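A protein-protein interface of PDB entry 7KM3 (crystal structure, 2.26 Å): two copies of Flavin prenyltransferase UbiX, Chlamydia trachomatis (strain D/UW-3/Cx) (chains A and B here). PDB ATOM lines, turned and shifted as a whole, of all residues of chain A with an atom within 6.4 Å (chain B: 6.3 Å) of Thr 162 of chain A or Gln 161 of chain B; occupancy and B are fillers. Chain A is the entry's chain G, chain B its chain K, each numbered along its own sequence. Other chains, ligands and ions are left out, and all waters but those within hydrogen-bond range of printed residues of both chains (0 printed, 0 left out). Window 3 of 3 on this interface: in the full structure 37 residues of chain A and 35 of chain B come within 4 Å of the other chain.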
ATOM      1  N   PRO A 160      16.992 -20.723 -25.369  1.00  0.00           N
ATOM      2  CA  PRO A 160      16.392 -19.388 -25.381  1.00  0.00           C
ATOM      3  C   PRO A 160      17.298 -18.376 -26.061  1.00  0.00           C
ATOM      4  O   PRO A 160      18.521 -18.532 -26.114  1.00  0.00           O
ATOM      5  CB  PRO A 160      16.224 -19.065 -23.890  1.00  0.00           C
ATOM      6  CG  PRO A 160      17.328 -19.841 -23.243  1.00  0.00           C
ATOM      7  CD  PRO A 160      17.380 -21.124 -24.003  1.00  0.00           C
ATOM      8  N   GLN A 161      16.677 -17.329 -26.584  1.00  0.00           N
ATOM      9  CA  GLN A 161      17.407 -16.229 -27.197  1.00  0.00           C
ATOM     10  C   GLN A 161      17.433 -14.995 -26.314  1.00  0.00           C
ATOM     11  O   GLN A 161      18.487 -14.371 -26.148  1.00  0.00           O
ATOM     12  CB  GLN A 161      16.782 -15.876 -28.547  1.00  0.00           C
ATOM     13  CG  GLN A 161      16.642 -17.064 -29.468  1.00  0.00           C
ATOM     14  CD  GLN A 161      17.983 -17.584 -29.937  1.00  0.00           C
ATOM     15  OE1 GLN A 161      18.923 -16.813 -30.135  1.00  0.00           O
ATOM     16  NE2 GLN A 161      18.080 -18.898 -30.116  1.00  0.00           N
ATOM     17  N   THR A 162      16.294 -14.651 -25.733  1.00  0.00           N
ATOM     18  CA  THR A 162      16.109 -13.424 -24.984  1.00  0.00           C
ATOM     19  C   THR A 162      15.912 -13.737 -23.512  1.00  0.00           C
ATOM     20  O   THR A 162      15.663 -14.880 -23.107  1.00  0.00           O
ATOM     21  CB  THR A 162      14.896 -12.639 -25.500  1.00  0.00           C
ATOM     22  OG1 THR A 162      13.705 -13.377 -25.195  1.00  0.00           O
ATOM     23  CG2 THR A 162      14.984 -12.405 -27.014  1.00  0.00           C
ATOM     24  N   ALA A 163      16.009 -12.681 -22.705  1.00  0.00           N
ATOM     25  CA  ALA A 163      15.650 -12.810 -21.303  1.00  0.00           C
ATOM     26  C   ALA A 163      14.176 -13.179 -21.156  1.00  0.00           C
ATOM     27  O   ALA A 163      13.820 -14.029 -20.331  1.00  0.00           O
ATOM     28  CB  ALA A 163      15.989 -11.514 -20.562  1.00  0.00           C
ATOM     29  N   GLU A 164      13.306 -12.576 -21.976  1.00  0.00           N
ATOM     30  CA  GLU A 164      11.891 -12.940 -21.947  1.00  0.00           C
ATOM     31  C   GLU A 164      11.688 -14.449 -22.099  1.00  0.00           C
ATOM     32  O   GLU A 164      10.840 -15.035 -21.417  1.00  0.00           O
ATOM     33  CB  GLU A 164      11.116 -12.187 -23.037  1.00  0.00           C
ATOM     34  CG  GLU A 164       9.652 -12.644 -23.115  1.00  0.00           C
ATOM     35  CD  GLU A 164       8.790 -11.869 -24.102  1.00  0.00           C
ATOM     36  OE1 GLU A 164       9.317 -11.360 -25.117  1.00  0.00           O
ATOM     37  OE2 GLU A 164       7.564 -11.795 -23.859  1.00  0.00           O
ATOM     38  N   ASP A 165      12.470 -15.096 -22.979  1.00  0.00           N
ATOM     39  CA  ASP A 165      12.326 -16.537 -23.211  1.00  0.00           C
ATOM     40  C   ASP A 165      12.591 -17.340 -21.944  1.00  0.00           C
ATOM     41  O   ASP A 165      11.852 -18.282 -21.626  1.00  0.00           O
ATOM     42  CB  ASP A 165      13.291 -17.015 -24.295  1.00  0.00           C
ATOM     43  CG  ASP A 165      12.956 -16.484 -25.658  1.00  0.00           C
ATOM     44  OD1 ASP A 165      11.758 -16.293 -25.960  1.00  0.00           O
ATOM     45  OD2 ASP A 165      13.911 -16.260 -26.429  1.00  0.00           O
ATOM     46  N   ILE A 166      13.682 -17.017 -21.247  1.00  0.00           N
ATOM     47  CA  ILE A 166      14.018 -17.735 -20.020  1.00  0.00           C
ATOM     48  C   ILE A 166      12.878 -17.614 -19.016  1.00  0.00           C
ATOM     49  O   ILE A 166      12.424 -18.614 -18.446  1.00  0.00           O
ATOM     50  CB  ILE A 166      15.360 -17.226 -19.462  1.00  0.00           C
ATOM     51  CG1 ILE A 166      16.501 -17.813 -20.309  1.00  0.00           C
ATOM     52  CG2 ILE A 166      15.502 -17.556 -17.963  1.00  0.00           C
ATOM     53  CD1 ILE A 166      17.795 -16.991 -20.334  1.00  0.00           C
ATOM     54  N   ALA A 167      12.340 -16.403 -18.857  1.00  0.00           N
ATOM     55  CA  ALA A 167      11.244 -16.179 -17.917  1.00  0.00           C
ATOM     56  C   ALA A 167       9.996 -16.959 -18.324  1.00  0.00           C
ATOM     57  O   ALA A 167       9.341 -17.595 -17.483  1.00  0.00           O
ATOM     58  CB  ALA A 167      10.942 -14.686 -17.822  1.00  0.00           C
ATOM     59  N   LYS B 159      18.513  -6.068 -14.939  1.00  0.00           N
ATOM     60  CA  LYS B 159      17.660  -5.791 -16.091  1.00  0.00           C
ATOM     61  C   LYS B 159      18.254  -6.389 -17.364  1.00  0.00           C
ATOM     62  O   LYS B 159      18.609  -5.659 -18.296  1.00  0.00           O
ATOM     63  CB  LYS B 159      17.447  -4.285 -16.257  1.00  0.00           C
ATOM     64  CG  LYS B 159      16.504  -3.677 -15.235  1.00  0.00           C
ATOM     65  CD  LYS B 159      16.216  -2.228 -15.563  1.00  0.00           C
ATOM     66  CE  LYS B 159      15.308  -1.581 -14.534  1.00  0.00           C
ATOM     67  NZ  LYS B 159      15.025  -0.181 -14.880  1.00  0.00           N
ATOM     68  N   PRO B 160      18.382  -7.706 -17.435  1.00  0.00           N
ATOM     69  CA  PRO B 160      18.938  -8.321 -18.639  1.00  0.00           C
ATOM     70  C   PRO B 160      17.940  -8.244 -19.775  1.00  0.00           C
ATOM     71  O   PRO B 160      16.730  -8.110 -19.581  1.00  0.00           O
ATOM     72  CB  PRO B 160      19.185  -9.769 -18.215  1.00  0.00           C
ATOM     73  CG  PRO B 160      18.108 -10.025 -17.193  1.00  0.00           C
ATOM     74  CD  PRO B 160      17.807  -8.704 -16.514  1.00  0.00           C
ATOM     75  N   GLN B 161      18.461  -8.328 -20.981  1.00  0.00           N
ATOM     76  CA  GLN B 161      17.568  -8.411 -22.116  1.00  0.00           C
ATOM     77  C   GLN B 161      17.816  -9.614 -23.006  1.00  0.00           C
ATOM     78  O   GLN B 161      16.861 -10.125 -23.584  1.00  0.00           O
ATOM     79  CB  GLN B 161      17.620  -7.101 -22.911  1.00  0.00           C
ATOM     80  CG  GLN B 161      16.887  -6.019 -22.137  1.00  0.00           C
ATOM     81  CD  GLN B 161      16.989  -4.654 -22.747  1.00  0.00           C
ATOM     82  OE1 GLN B 161      17.640  -4.467 -23.774  1.00  0.00           O
ATOM     83  NE2 GLN B 161      16.339  -3.677 -22.119  1.00  0.00           N
ATOM     84  N   THR B 162      19.039 -10.119 -23.090  1.00  0.00           N
ATOM     85  CA  THR B 162      19.269 -11.334 -23.851  1.00  0.00           C
ATOM     86  C   THR B 162      19.477 -12.504 -22.903  1.00  0.00           C
ATOM     87  O   THR B 162      19.704 -12.339 -21.702  1.00  0.00           O
ATOM     88  CB  THR B 162      20.468 -11.198 -24.797  1.00  0.00           C
ATOM     89  OG1 THR B 162      21.671 -11.018 -24.037  1.00  0.00           O
ATOM     90  CG2 THR B 162      20.275 -10.013 -25.753  1.00  0.00           C
ATOM     91  N   ALA B 163      19.374 -13.706 -23.467  1.00  0.00           N
ATOM     92  CA  ALA B 163      19.770 -14.886 -22.714  1.00  0.00           C
ATOM     93  C   ALA B 163      21.236 -14.787 -22.313  1.00  0.00           C
ATOM     94  O   ALA B 163      21.596 -15.085 -21.168  1.00  0.00           O
ATOM     95  CB  ALA B 163      19.506 -16.145 -23.540  1.00  0.00           C
ATOM     96  N   GLU B 164      22.087 -14.327 -23.240  1.00  0.00           N
ATOM     97  CA  GLU B 164      23.508 -14.164 -22.949  1.00  0.00           C
ATOM     98  C   GLU B 164      23.735 -13.260 -21.739  1.00  0.00           C
ATOM     99  O   GLU B 164      24.659 -13.491 -20.951  1.00  0.00           O
ATOM    100  CB  GLU B 164      24.241 -13.598 -24.172  1.00  0.00           C
ATOM    101  CG  GLU B 164      25.763 -13.555 -23.998  1.00  0.00           C
ATOM    102  CD  GLU B 164      26.479 -12.697 -25.037  1.00  0.00           C
ATOM    103  OE1 GLU B 164      27.415 -11.957 -24.653  1.00  0.00           O
ATOM    104  OE2 GLU B 164      26.118 -12.758 -26.232  1.00  0.00           O
ATOM    105  N   ASP B 165      22.919 -12.214 -21.589  1.00  0.00           N
ATOM    106  CA  ASP B 165      23.054 -11.340 -20.429  1.00  0.00           C
ATOM    107  C   ASP B 165      22.838 -12.115 -19.133  1.00  0.00           C
ATOM    108  O   ASP B 165      23.523 -11.865 -18.135  1.00  0.00           O
ATOM    109  CB  ASP B 165      22.064 -10.171 -20.505  1.00  0.00           C
ATOM    110  CG  ASP B 165      22.255  -9.302 -21.747  1.00  0.00           C
ATOM    111  OD1 ASP B 165      23.390  -9.212 -22.270  1.00  0.00           O
ATOM    112  OD2 ASP B 165      21.252  -8.703 -22.199  1.00  0.00           O
ATOM    113  N   ILE B 166      21.882 -13.045 -19.124  1.00  0.00           N
ATOM    114  CA  ILE B 166      21.583 -13.778 -17.896  1.00  0.00           C
ATOM    115  C   ILE B 166      22.688 -14.778 -17.586  1.00  0.00           C
ATOM    116  O   ILE B 166      23.129 -14.889 -16.440  1.00  0.00           O
ATOM    117  CB  ILE B 166      20.200 -14.446 -17.985  1.00  0.00           C
ATOM    118  CG1 ILE B 166      19.116 -13.388 -17.777  1.00  0.00           C
ATOM    119  CG2 ILE B 166      20.075 -15.575 -16.965  1.00  0.00           C
ATOM    120  CD1 ILE B 166      17.712 -13.865 -18.010  1.00  0.00           C
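N of Gln 161 of chain A lies within hydrogen-bond range of OD2 of Asp 165 of chain A, at 3.0 Å.
The side-chain hydroxyl of Thr 162 of chain A sits close to the backbone NH of Glu 164 of chain A (3.3 Å).
The side-chain carboxylate (OD2) of Asp 165 of chain A is in hydrogen-bond range of the backbone NH (N) of Thr 162 of chain A, 3.0 Å away.
The backbone NH (N) of Gln 161 of chain B is in hydrogen-bond range of the side-chain carboxylate (OD2) of Asp 165 of chain B (3.1 Å).
The backbone NH (N) of Glu 164 of chain B sits close to the side-chain hydroxyl (OG1) of Thr 162 of chain B (3.4 Å).
The backbone NH (N) of Thr 162 of chain B sits at hydrogen-bond distance from the side-chain carboxylate (OD2) of Asp 165 of chain B.
O of Gln 161 of chain A lies within hydrogen-bond range of N of Ala 163 of chain B (2.9 Å).
The backbone carbonyl oxygen (O) of Gln 161 of chain B sits at hydrogen-bond distance from the backbone NH (N) of Ala 163 of chain A.
Among the printed residues, merely in contact across the chains: Pro 160 of chain A with Ala 163 of chain B (3.6 Å), Gln 161 of chain A with Thr 162 of chain B (3.9 Å), Thr 162 of chain A with Gln 161 of chain B (3.7 Å), Thr 162 of chain A with Thr 162 of chain B (3.8 Å), Thr 162 of chain A with Ala 163 of chain B (3.5 Å), Ala 163 of chain A with Pro 160 of chain B (3.6 Å), Ala 163 of chain A with Thr 162 of chain B (3.5 Å), Ala 163 of chain A with Ala 163 of chain B (3.6 Å), Ala 163 of chain A with Ile 166 of chain B (3.9 Å), Ile 166 of chain A with Ala 163 of chain B (3.7 Å) and Ile 166 of chain A with Ile 166 of chain B (3.9 Å).
Of the 8 printed residues of chain A, 5 touch a printed residue of chain B.
Hydrophobic or aromatic side chains of chain A that line the printed part of chain B: Ala 163 and Ile 166.
Of the 8 printed residues of chain B, 5 touch a printed residue of chain A.
Hydrophobic or aromatic side chains of chain B that line the printed part of chain A: Ala 163 and Ile 166.
Thr 162 of chain A touches three residues of chain B.
Printed residues of chain B within 4 Å of Ala 163 of chain A: Pro 160 (3.6 Å), Gln 161 (2.8 Å), Thr 162 (3.5 Å), Ala 163 (3.6 Å) and Ile 166 (3.9 Å).
Glu 164 of chain A touches none of the printed residues of chain B.
Printed residues of chain B within 4 Å of Ile 166 of chain A: Ala 163 and Ile 166.
Printed residues of chain A within 4 Å of Pro 160 of chain B: Ala 163 (3.6 Å).
Of the printed residues of chain A, Ile 166 of chain B touches Ala 163 and Ile 166.
The nearest residue of chain A that does not touch Gln 161 of chain B is Glu 164 of chain A (4.6 Å).
The nearest printed residue of chain A that does not touch Pro 160 of chain B is Glu 164 of chain A (6.1 Å).
Pro 160 of chain A touches Ala 163 of chain B, and with the chains exchanged Ala 163 of chain A touches Pro 160 of chain B.
Gln 161 of chain A touches Thr 162 of chain B, and with the chains exchanged Thr 162 of chain A touches Gln 161 of chain B.
Gln 161 of chain A touches Ala 163 of chain B, and with the chains exchanged Ala 163 of chain A touches Gln 161 of chain B.
Ala 163 of chain A touches Ile 166 of chain B, and with the chains exchanged Ile 166 of chain A touches Ala 163 of chain B.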
